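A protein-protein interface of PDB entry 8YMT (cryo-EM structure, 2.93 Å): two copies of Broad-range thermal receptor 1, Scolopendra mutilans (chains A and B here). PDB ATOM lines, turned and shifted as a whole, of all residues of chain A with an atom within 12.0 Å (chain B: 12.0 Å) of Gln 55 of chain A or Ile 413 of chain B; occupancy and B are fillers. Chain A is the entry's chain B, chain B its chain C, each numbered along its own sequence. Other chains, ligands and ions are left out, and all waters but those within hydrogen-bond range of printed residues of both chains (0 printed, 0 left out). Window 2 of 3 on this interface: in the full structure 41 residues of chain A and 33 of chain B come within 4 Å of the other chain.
OE1 of Gln 55 of chain A sits close to NH1 of Arg 53 of chain A.
Hydrophobic or aromatic side chains of chain B that line the printed part of chain A: Leu 403, Ile 406 and Ile 413.
Hydrophobic or aromatic side chains of chain A within 4 Å of the printed part of chain B: Leu 58 and Trp 59.
Among the printed residues, 9 pairs touch across the chains.
Among the printed residues, no Asp or Glu carboxylate lies within 4 Å of a Lys or Arg side-chain nitrogen of the other chain.
No position is printed for both chains.
Of the 9 pairs that touch across the chains among the printed residues, none has its exchanged pair printed and touching as well.
Of chain B, only Glu 410 (3.2 Å), Ile 413 (2.9 Å) and Phe 414 (3.0 Å) come within 4 Å of Gln 55 of chain A.
Ile 413 of chain B touches just one residue of chain A: Gln 55.
No residue of chain B comes within 4 Å of Arg 53 of chain A.
No residue of chain B comes within 4 Å of Trp 54 of chain A.
No residue of chain B comes within 4 Å of Arg 56 of chain A.
Ala 57 of chain A touches none of the printed residues of chain B.
Glu 410 of chain B touches just these residues of chain A: Gln 55, Leu 58, Trp 59 and Gly 62.
No residue of chain A comes within 4 Å of Val 412 of chain B.
Of chain A, only Gln 55 comes within 4 Å of Phe 414 of chain B.
Of the printed residues of chain A, Ile 406 of chain B touches Gly 62.
Of the printed residues of chain B, Trp 59 of chain A touches Glu 407 and Glu 410.
Phe 409 of chain B touches none of the printed residues of chain A.
Phe 60 of chain A touches none of the printed residues of chain B.
The nearest residue of chain A that does not touch Ile 413 of chain B is Leu 58 of chain A (4.5 Å).
NE2 of Gln 55 of chain A sits at hydrogen-bond distance from O of Glu 410 of chain B, 3.2 Å away.
The backbone carbonyl oxygen (O) of Ile 413 of chain B sits at hydrogen-bond distance from the side-chain amide nitrogen (NE2) of Gln 55 of chain A (2.9 Å).
The backbone carbonyl oxygen (O) of Leu 58 of chain A lies close to the side-chain carboxylate (OE2) of Glu 410 of chain B (3.1 Å).
Among the printed residues, pairs that only touch across the chains: Trp 59 of chain A with Glu 410 of chain B, Gln 55 of chain A with Phe 414 of chain B, Trp 59 of chain A with Glu 407 of chain B, Gly 62 of chain A with Glu 410 of chain B, Gly 62 of chain A with Ile 406 of chain B and Gly 62 of chain A with Leu 403 of chain B.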
ATOM      1  N   ARG A  53      26.265  16.256  14.305  1.00  0.00           N
ATOM      2  CA  ARG A  53      27.040  17.079  13.382  1.00  0.00           C
ATOM      3  C   ARG A  53      26.208  17.465  12.160  1.00  0.00           C
ATOM      4  O   ARG A  53      25.040  17.831  12.289  1.00  0.00           O
ATOM      5  CB  ARG A  53      28.319  16.347  12.961  1.00  0.00           C
ATOM      6  CG  ARG A  53      28.116  14.899  12.529  1.00  0.00           C
ATOM      7  CD  ARG A  53      28.084  14.757  11.017  1.00  0.00           C
ATOM      8  NE  ARG A  53      28.123  13.362  10.596  1.00  0.00           N
ATOM      9  CZ  ARG A  53      28.009  12.954   9.340  1.00  0.00           C
ATOM     10  NH1 ARG A  53      27.854  13.815   8.346  1.00  0.00           N
ATOM     11  NH2 ARG A  53      28.051  11.653   9.072  1.00  0.00           N
ATOM     12  N   TRP A  54      26.820  17.389  10.979  1.00  0.00           N
ATOM     13  CA  TRP A  54      26.151  17.750   9.735  1.00  0.00           C
ATOM     14  C   TRP A  54      24.792  17.075   9.605  1.00  0.00           C
ATOM     15  O   TRP A  54      23.761  17.748   9.501  1.00  0.00           O
ATOM     16  CB  TRP A  54      27.016  17.375   8.529  1.00  0.00           C
ATOM     17  CG  TRP A  54      28.320  18.103   8.445  1.00  0.00           C
ATOM     18  CD1 TRP A  54      28.714  19.174   9.191  1.00  0.00           C
ATOM     19  CD2 TRP A  54      29.406  17.809   7.557  1.00  0.00           C
ATOM     20  NE1 TRP A  54      29.979  19.566   8.824  1.00  0.00           N
ATOM     21  CE2 TRP A  54      30.426  18.743   7.823  1.00  0.00           C
ATOM     22  CE3 TRP A  54      29.614  16.847   6.565  1.00  0.00           C
ATOM     23  CZ2 TRP A  54      31.636  18.743   7.132  1.00  0.00           C
ATOM     24  CZ3 TRP A  54      30.815  16.847   5.880  1.00  0.00           C
ATOM     25  CH2 TRP A  54      31.811  17.790   6.167  1.00  0.00           C
ATOM     26  N   GLN A  55      24.784  15.740   9.619  1.00  0.00           N
ATOM     27  CA  GLN A  55      23.573  15.008   9.261  1.00  0.00           C
ATOM     28  C   GLN A  55      22.500  15.137  10.334  1.00  0.00           C
ATOM     29  O   GLN A  55      21.324  15.352  10.019  1.00  0.00           O
ATOM     30  CB  GLN A  55      23.908  13.541   9.003  1.00  0.00           C
ATOM     31  CG  GLN A  55      24.858  13.342   7.838  1.00  0.00           C
ATOM     32  CD  GLN A  55      24.552  14.273   6.680  1.00  0.00           C
ATOM     33  OE1 GLN A  55      25.369  15.119   6.318  1.00  0.00           O
ATOM     34  NE2 GLN A  55      23.364  14.134   6.106  1.00  0.00           N
ATOM     35  N   ARG A  56      22.878  15.004  11.607  1.00  0.00           N
ATOM     36  CA  ARG A  56      21.901  15.180  12.674  1.00  0.00           C
ATOM     37  C   ARG A  56      21.363  16.603  12.731  1.00  0.00           C
ATOM     38  O   ARG A  56      20.161  16.792  12.948  1.00  0.00           O
ATOM     39  CB  ARG A  56      22.513  14.794  14.023  1.00  0.00           C
ATOM     40  CG  ARG A  56      21.586  15.022  15.206  1.00  0.00           C
ATOM     41  CD  ARG A  56      20.375  14.103  15.149  1.00  0.00           C
ATOM     42  NE  ARG A  56      20.615  12.831  15.823  1.00  0.00           N
ATOM     43  CZ  ARG A  56      20.337  11.644  15.301  1.00  0.00           C
ATOM     44  NH1 ARG A  56      19.806  11.525  14.094  1.00  0.00           N
ATOM     45  NH2 ARG A  56      20.599  10.548  16.007  1.00  0.00           N
ATOM     46  N   ALA A  57      22.223  17.606  12.531  1.00  0.00           N
ATOM     47  CA  ALA A  57      21.749  18.984  12.500  1.00  0.00           C
ATOM     48  C   ALA A  57      20.781  19.208  11.346  1.00  0.00           C
ATOM     49  O   ALA A  57      19.766  19.895  11.505  1.00  0.00           O
ATOM     50  CB  ALA A  57      22.933  19.945  12.402  1.00  0.00           C
ATOM     51  N   LEU A  58      21.073  18.635  10.176  1.00  0.00           N
ATOM     52  CA  LEU A  58      20.181  18.814   9.036  1.00  0.00           C
ATOM     53  C   LEU A  58      18.862  18.079   9.252  1.00  0.00           C
ATOM     54  O   LEU A  58      17.802  18.554   8.829  1.00  0.00           O
ATOM     55  CB  LEU A  58      20.870  18.348   7.753  1.00  0.00           C
ATOM     56  CG  LEU A  58      20.154  18.646   6.434  1.00  0.00           C
ATOM     57  CD1 LEU A  58      21.158  18.757   5.295  1.00  0.00           C
ATOM     58  CD2 LEU A  58      19.110  17.597   6.124  1.00  0.00           C
ATOM     59  N   TRP A  59      18.905  16.917   9.907  1.00  0.00           N
ATOM     60  CA  TRP A  59      17.673  16.220  10.268  1.00  0.00           C
ATOM     61  C   TRP A  59      16.837  17.056  11.228  1.00  0.00           C
ATOM     62  O   TRP A  59      15.610  17.139  11.095  1.00  0.00           O
ATOM     63  CB  TRP A  59      17.997  14.860  10.886  1.00  0.00           C
ATOM     64  CG  TRP A  59      16.794  14.147  11.435  1.00  0.00           C
ATOM     65  CD1 TRP A  59      15.814  13.522  10.723  1.00  0.00           C
ATOM     66  CD2 TRP A  59      16.442  13.995  12.817  1.00  0.00           C
ATOM     67  NE1 TRP A  59      14.877  12.986  11.572  1.00  0.00           N
ATOM     68  CE2 TRP A  59      15.241  13.263  12.864  1.00  0.00           C
ATOM     69  CE3 TRP A  59      17.030  14.405  14.019  1.00  0.00           C
ATOM     70  CZ2 TRP A  59      14.612  12.933  14.064  1.00  0.00           C
ATOM     71  CZ3 TRP A  59      16.405  14.077  15.209  1.00  0.00           C
ATOM     72  CH2 TRP A  59      15.209  13.347  15.222  1.00  0.00           C
ATOM     73  N   PHE A  60      17.489  17.673  12.214  1.00  0.00           N
ATOM     74  CA  PHE A  60      16.778  18.558  13.129  1.00  0.00           C
ATOM     75  C   PHE A  60      16.158  19.728  12.378  1.00  0.00           C
ATOM     76  O   PHE A  60      15.019  20.123  12.646  1.00  0.00           O
ATOM     77  CB  PHE A  60      17.729  19.058  14.218  1.00  0.00           C
ATOM     78  CG  PHE A  60      17.106  20.044  15.163  1.00  0.00           C
ATOM     79  CD1 PHE A  60      16.326  19.614  16.223  1.00  0.00           C
ATOM     80  CD2 PHE A  60      17.298  21.405  14.990  1.00  0.00           C
ATOM     81  CE1 PHE A  60      15.751  20.521  17.093  1.00  0.00           C
ATOM     82  CE2 PHE A  60      16.726  22.317  15.856  1.00  0.00           C
ATOM     83  CZ  PHE A  60      15.952  21.875  16.910  1.00  0.00           C
ATOM     84  N   ALA A  61      16.903  20.299  11.430  1.00  0.00           N
ATOM     85  CA  ALA A  61      16.380  21.404  10.634  1.00  0.00           C
ATOM     86  C   ALA A  61      15.152  20.971   9.841  1.00  0.00           C
ATOM     87  O   ALA A  61      14.145  21.682   9.791  1.00  0.00           O
ATOM     88  CB  ALA A  61      17.465  21.934   9.697  1.00  0.00           C
ATOM     89  N   GLY A  62      15.222  19.796   9.211  1.00  0.00           N
ATOM     90  CA  GLY A  62      14.082  19.297   8.465  1.00  0.00           C
ATOM     91  C   GLY A  62      12.870  19.040   9.337  1.00  0.00           C
ATOM     92  O   GLY A  62      11.745  19.385   8.960  1.00  0.00           O
ATOM     93  N   VAL A  63      13.074  18.439  10.509  1.00  0.00           N
ATOM     94  CA  VAL A  63      11.961  18.180  11.415  1.00  0.00           C
ATOM     95  C   VAL A  63      11.342  19.484  11.898  1.00  0.00           C
ATOM     96  O   VAL A  63      10.113  19.618  11.953  1.00  0.00           O
ATOM     97  CB  VAL A  63      12.423  17.301  12.590  1.00  0.00           C
ATOM     98  CG1 VAL A  63      11.293  17.122  13.592  1.00  0.00           C
ATOM     99  CG2 VAL A  63      12.906  15.952  12.081  1.00  0.00           C
ATOM    100  N   VAL A  64      12.172  20.465  12.262  1.00  0.00           N
ATOM    101  CA  VAL A  64      11.646  21.743  12.726  1.00  0.00           C
ATOM    102  C   VAL A  64      10.884  22.439  11.608  1.00  0.00           C
ATOM    103  O   VAL A  64       9.835  23.048  11.838  1.00  0.00           O
ATOM    104  CB  VAL A  64      12.778  22.629  13.280  1.00  0.00           C
ATOM    105  CG1 VAL A  64      13.734  23.036  12.177  1.00  0.00           C
ATOM    106  CG2 VAL A  64      12.197  23.857  13.967  1.00  0.00           C
ATOM    107  N   LEU B 403       7.885  15.330   5.149  1.00  0.00           N
ATOM    108  CA  LEU B 403       8.980  15.038   6.065  1.00  0.00           C
ATOM    109  C   LEU B 403       9.673  13.738   5.678  1.00  0.00           C
ATOM    110  O   LEU B 403      10.881  13.586   5.886  1.00  0.00           O
ATOM    111  CB  LEU B 403       8.477  14.965   7.505  1.00  0.00           C
ATOM    112  CG  LEU B 403       9.558  14.595   8.525  1.00  0.00           C
ATOM    113  CD1 LEU B 403      10.696  15.607   8.491  1.00  0.00           C
ATOM    114  CD2 LEU B 403       8.981  14.479   9.923  1.00  0.00           C
ATOM    115  N   SER B 404       8.925  12.793   5.107  1.00  0.00           N
ATOM    116  CA  SER B 404       9.541  11.556   4.638  1.00  0.00           C
ATOM    117  C   SER B 404      10.545  11.829   3.524  1.00  0.00           C
ATOM    118  O   SER B 404      11.659  11.296   3.541  1.00  0.00           O
ATOM    119  CB  SER B 404       8.465  10.579   4.167  1.00  0.00           C
ATOM    120  OG  SER B 404       7.649  10.161   5.247  1.00  0.00           O
ATOM    121  N   VAL B 405      10.174  12.664   2.550  1.00  0.00           N
ATOM    122  CA  VAL B 405      11.110  12.987   1.477  1.00  0.00           C
ATOM    123  C   VAL B 405      12.281  13.796   2.010  1.00  0.00           C
ATOM    124  O   VAL B 405      13.422  13.620   1.562  1.00  0.00           O
ATOM    125  CB  VAL B 405      10.401  13.724   0.325  1.00  0.00           C
ATOM    126  CG1 VAL B 405       9.344  12.839  -0.293  1.00  0.00           C
ATOM    127  CG2 VAL B 405       9.796  15.026   0.810  1.00  0.00           C
ATOM    128  N   ILE B 406      12.034  14.697   2.964  1.00  0.00           N
ATOM    129  CA  ILE B 406      13.139  15.428   3.571  1.00  0.00           C
ATOM    130  C   ILE B 406      14.117  14.490   4.268  1.00  0.00           C
ATOM    131  O   ILE B 406      15.332  14.651   4.113  1.00  0.00           O
ATOM    132  CB  ILE B 406      12.625  16.486   4.559  1.00  0.00           C
ATOM    133  CG1 ILE B 406      11.688  17.462   3.849  1.00  0.00           C
ATOM    134  CG2 ILE B 406      13.789  17.232   5.190  1.00  0.00           C
ATOM    135  CD1 ILE B 406      12.332  18.190   2.689  1.00  0.00           C
ATOM    136  N   GLU B 407      13.620  13.509   5.024  1.00  0.00           N
ATOM    137  CA  GLU B 407      14.503  12.549   5.678  1.00  0.00           C
ATOM    138  C   GLU B 407      15.227  11.676   4.659  1.00  0.00           C
ATOM    139  O   GLU B 407      16.392  11.312   4.860  1.00  0.00           O
ATOM    140  CB  GLU B 407      13.710  11.688   6.658  1.00  0.00           C
ATOM    141  CG  GLU B 407      13.129  12.457   7.835  1.00  0.00           C
ATOM    142  CD  GLU B 407      12.281  11.586   8.741  1.00  0.00           C
ATOM    143  OE1 GLU B 407      12.030  10.417   8.380  1.00  0.00           O
ATOM    144  OE2 GLU B 407      11.867  12.070   9.816  1.00  0.00           O
ATOM    145  N   VAL B 408      14.551  11.315   3.566  1.00  0.00           N
ATOM    146  CA  VAL B 408      15.204  10.529   2.523  1.00  0.00           C
ATOM    147  C   VAL B 408      16.356  11.315   1.913  1.00  0.00           C
ATOM    148  O   VAL B 408      17.449  10.776   1.695  1.00  0.00           O
ATOM    149  CB  VAL B 408      14.182  10.097   1.457  1.00  0.00           C
ATOM    150  CG1 VAL B 408      14.884   9.383   0.312  1.00  0.00           C
ATOM    151  CG2 VAL B 408      13.119   9.202   2.074  1.00  0.00           C
ATOM    152  N   PHE B 409      16.134  12.599   1.628  1.00  0.00           N
ATOM    153  CA  PHE B 409      17.216  13.438   1.122  1.00  0.00           C
ATOM    154  C   PHE B 409      18.328  13.590   2.151  1.00  0.00           C
ATOM    155  O   PHE B 409      19.510  13.615   1.788  1.00  0.00           O
ATOM    156  CB  PHE B 409      16.675  14.807   0.711  1.00  0.00           C
ATOM    157  CG  PHE B 409      16.288  14.896  -0.735  1.00  0.00           C
ATOM    158  CD1 PHE B 409      17.032  15.658  -1.620  1.00  0.00           C
ATOM    159  CD2 PHE B 409      15.181  14.215  -1.214  1.00  0.00           C
ATOM    160  CE1 PHE B 409      16.679  15.740  -2.953  1.00  0.00           C
ATOM    161  CE2 PHE B 409      14.822  14.295  -2.545  1.00  0.00           C
ATOM    162  CZ  PHE B 409      15.573  15.058  -3.416  1.00  0.00           C
ATOM    163  N   GLU B 410      17.971  13.699   3.432  1.00  0.00           N
ATOM    164  CA  GLU B 410      18.980  13.733   4.485  1.00  0.00           C
ATOM    165  C   GLU B 410      19.858  12.491   4.435  1.00  0.00           C
ATOM    166  O   GLU B 410      21.089  12.585   4.508  1.00  0.00           O
ATOM    167  CB  GLU B 410      18.302  13.847   5.851  1.00  0.00           C
ATOM    168  CG  GLU B 410      17.438  15.082   6.019  1.00  0.00           C
ATOM    169  CD  GLU B 410      16.707  15.102   7.343  1.00  0.00           C
ATOM    170  OE1 GLU B 410      16.695  14.059   8.029  1.00  0.00           O
ATOM    171  OE2 GLU B 410      16.141  16.158   7.699  1.00  0.00           O
ATOM    172  N   VAL B 411      19.235  11.316   4.312  1.00  0.00           N
ATOM    173  CA  VAL B 411      19.994  10.076   4.195  1.00  0.00           C
ATOM    174  C   VAL B 411      20.804  10.065   2.907  1.00  0.00           C
ATOM    175  O   VAL B 411      21.856   9.416   2.832  1.00  0.00           O
ATOM    176  CB  VAL B 411      19.051   8.862   4.280  1.00  0.00           C
ATOM    177  CG1 VAL B 411      19.809   7.579   3.978  1.00  0.00           C
ATOM    178  CG2 VAL B 411      18.399   8.793   5.653  1.00  0.00           C
ATOM    179  N   VAL B 412      20.337  10.770   1.874  1.00  0.00           N
ATOM    180  CA  VAL B 412      21.103  10.866   0.634  1.00  0.00           C
ATOM    181  C   VAL B 412      22.467  11.486   0.903  1.00  0.00           C
ATOM    182  O   VAL B 412      23.493  11.011   0.404  1.00  0.00           O
ATOM    183  CB  VAL B 412      20.315  11.665  -0.422  1.00  0.00           C
ATOM    184  CG1 VAL B 412      21.164  11.881  -1.665  1.00  0.00           C
ATOM    185  CG2 VAL B 412      19.021  10.949  -0.773  1.00  0.00           C
ATOM    186  N   ILE B 413      22.498  12.554   1.696  1.00  0.00           N
ATOM    187  CA  ILE B 413      23.750  13.154   2.139  1.00  0.00           C
ATOM    188  C   ILE B 413      24.160  12.466   3.436  1.00  0.00           C
ATOM    189  O   ILE B 413      25.071  12.920   4.138  1.00  0.00           O
ATOM    190  CB  ILE B 413      23.612  14.678   2.317  1.00  0.00           C
ATOM    191  CG1 ILE B 413      24.954  15.304   2.707  1.00  0.00           C
ATOM    192  CG2 ILE B 413      22.539  15.003   3.344  1.00  0.00           C
ATOM    193  CD1 ILE B 413      24.965  16.817   2.644  1.00  0.00           C
ATOM    194  N   PHE B 414      23.480  11.368   3.757  1.00  0.00           N
ATOM    195  CA  PHE B 414      23.779  10.555   4.933  1.00  0.00           C
ATOM    196  C   PHE B 414      23.228  11.186   6.205  1.00  0.00           C
ATOM    197  O   PHE B 414      22.271  10.684   6.795  1.00  0.00           O
ATOM    198  CB  PHE B 414      25.287  10.333   5.066  1.00  0.00           C
ATOM    199  CG  PHE B 414      25.846   9.361   4.066  1.00  0.00           C
ATOM    200  CD1 PHE B 414      25.002   8.550   3.325  1.00  0.00           C
ATOM    201  CD2 PHE B 414      27.211   9.261   3.866  1.00  0.00           C
ATOM    202  CE1 PHE B 414      25.511   7.656   2.402  1.00  0.00           C
ATOM    203  CE2 PHE B 414      27.727   8.367   2.946  1.00  0.00           C
ATOM    204  CZ  PHE B 414      26.875   7.564   2.213  1.00  0.00           C
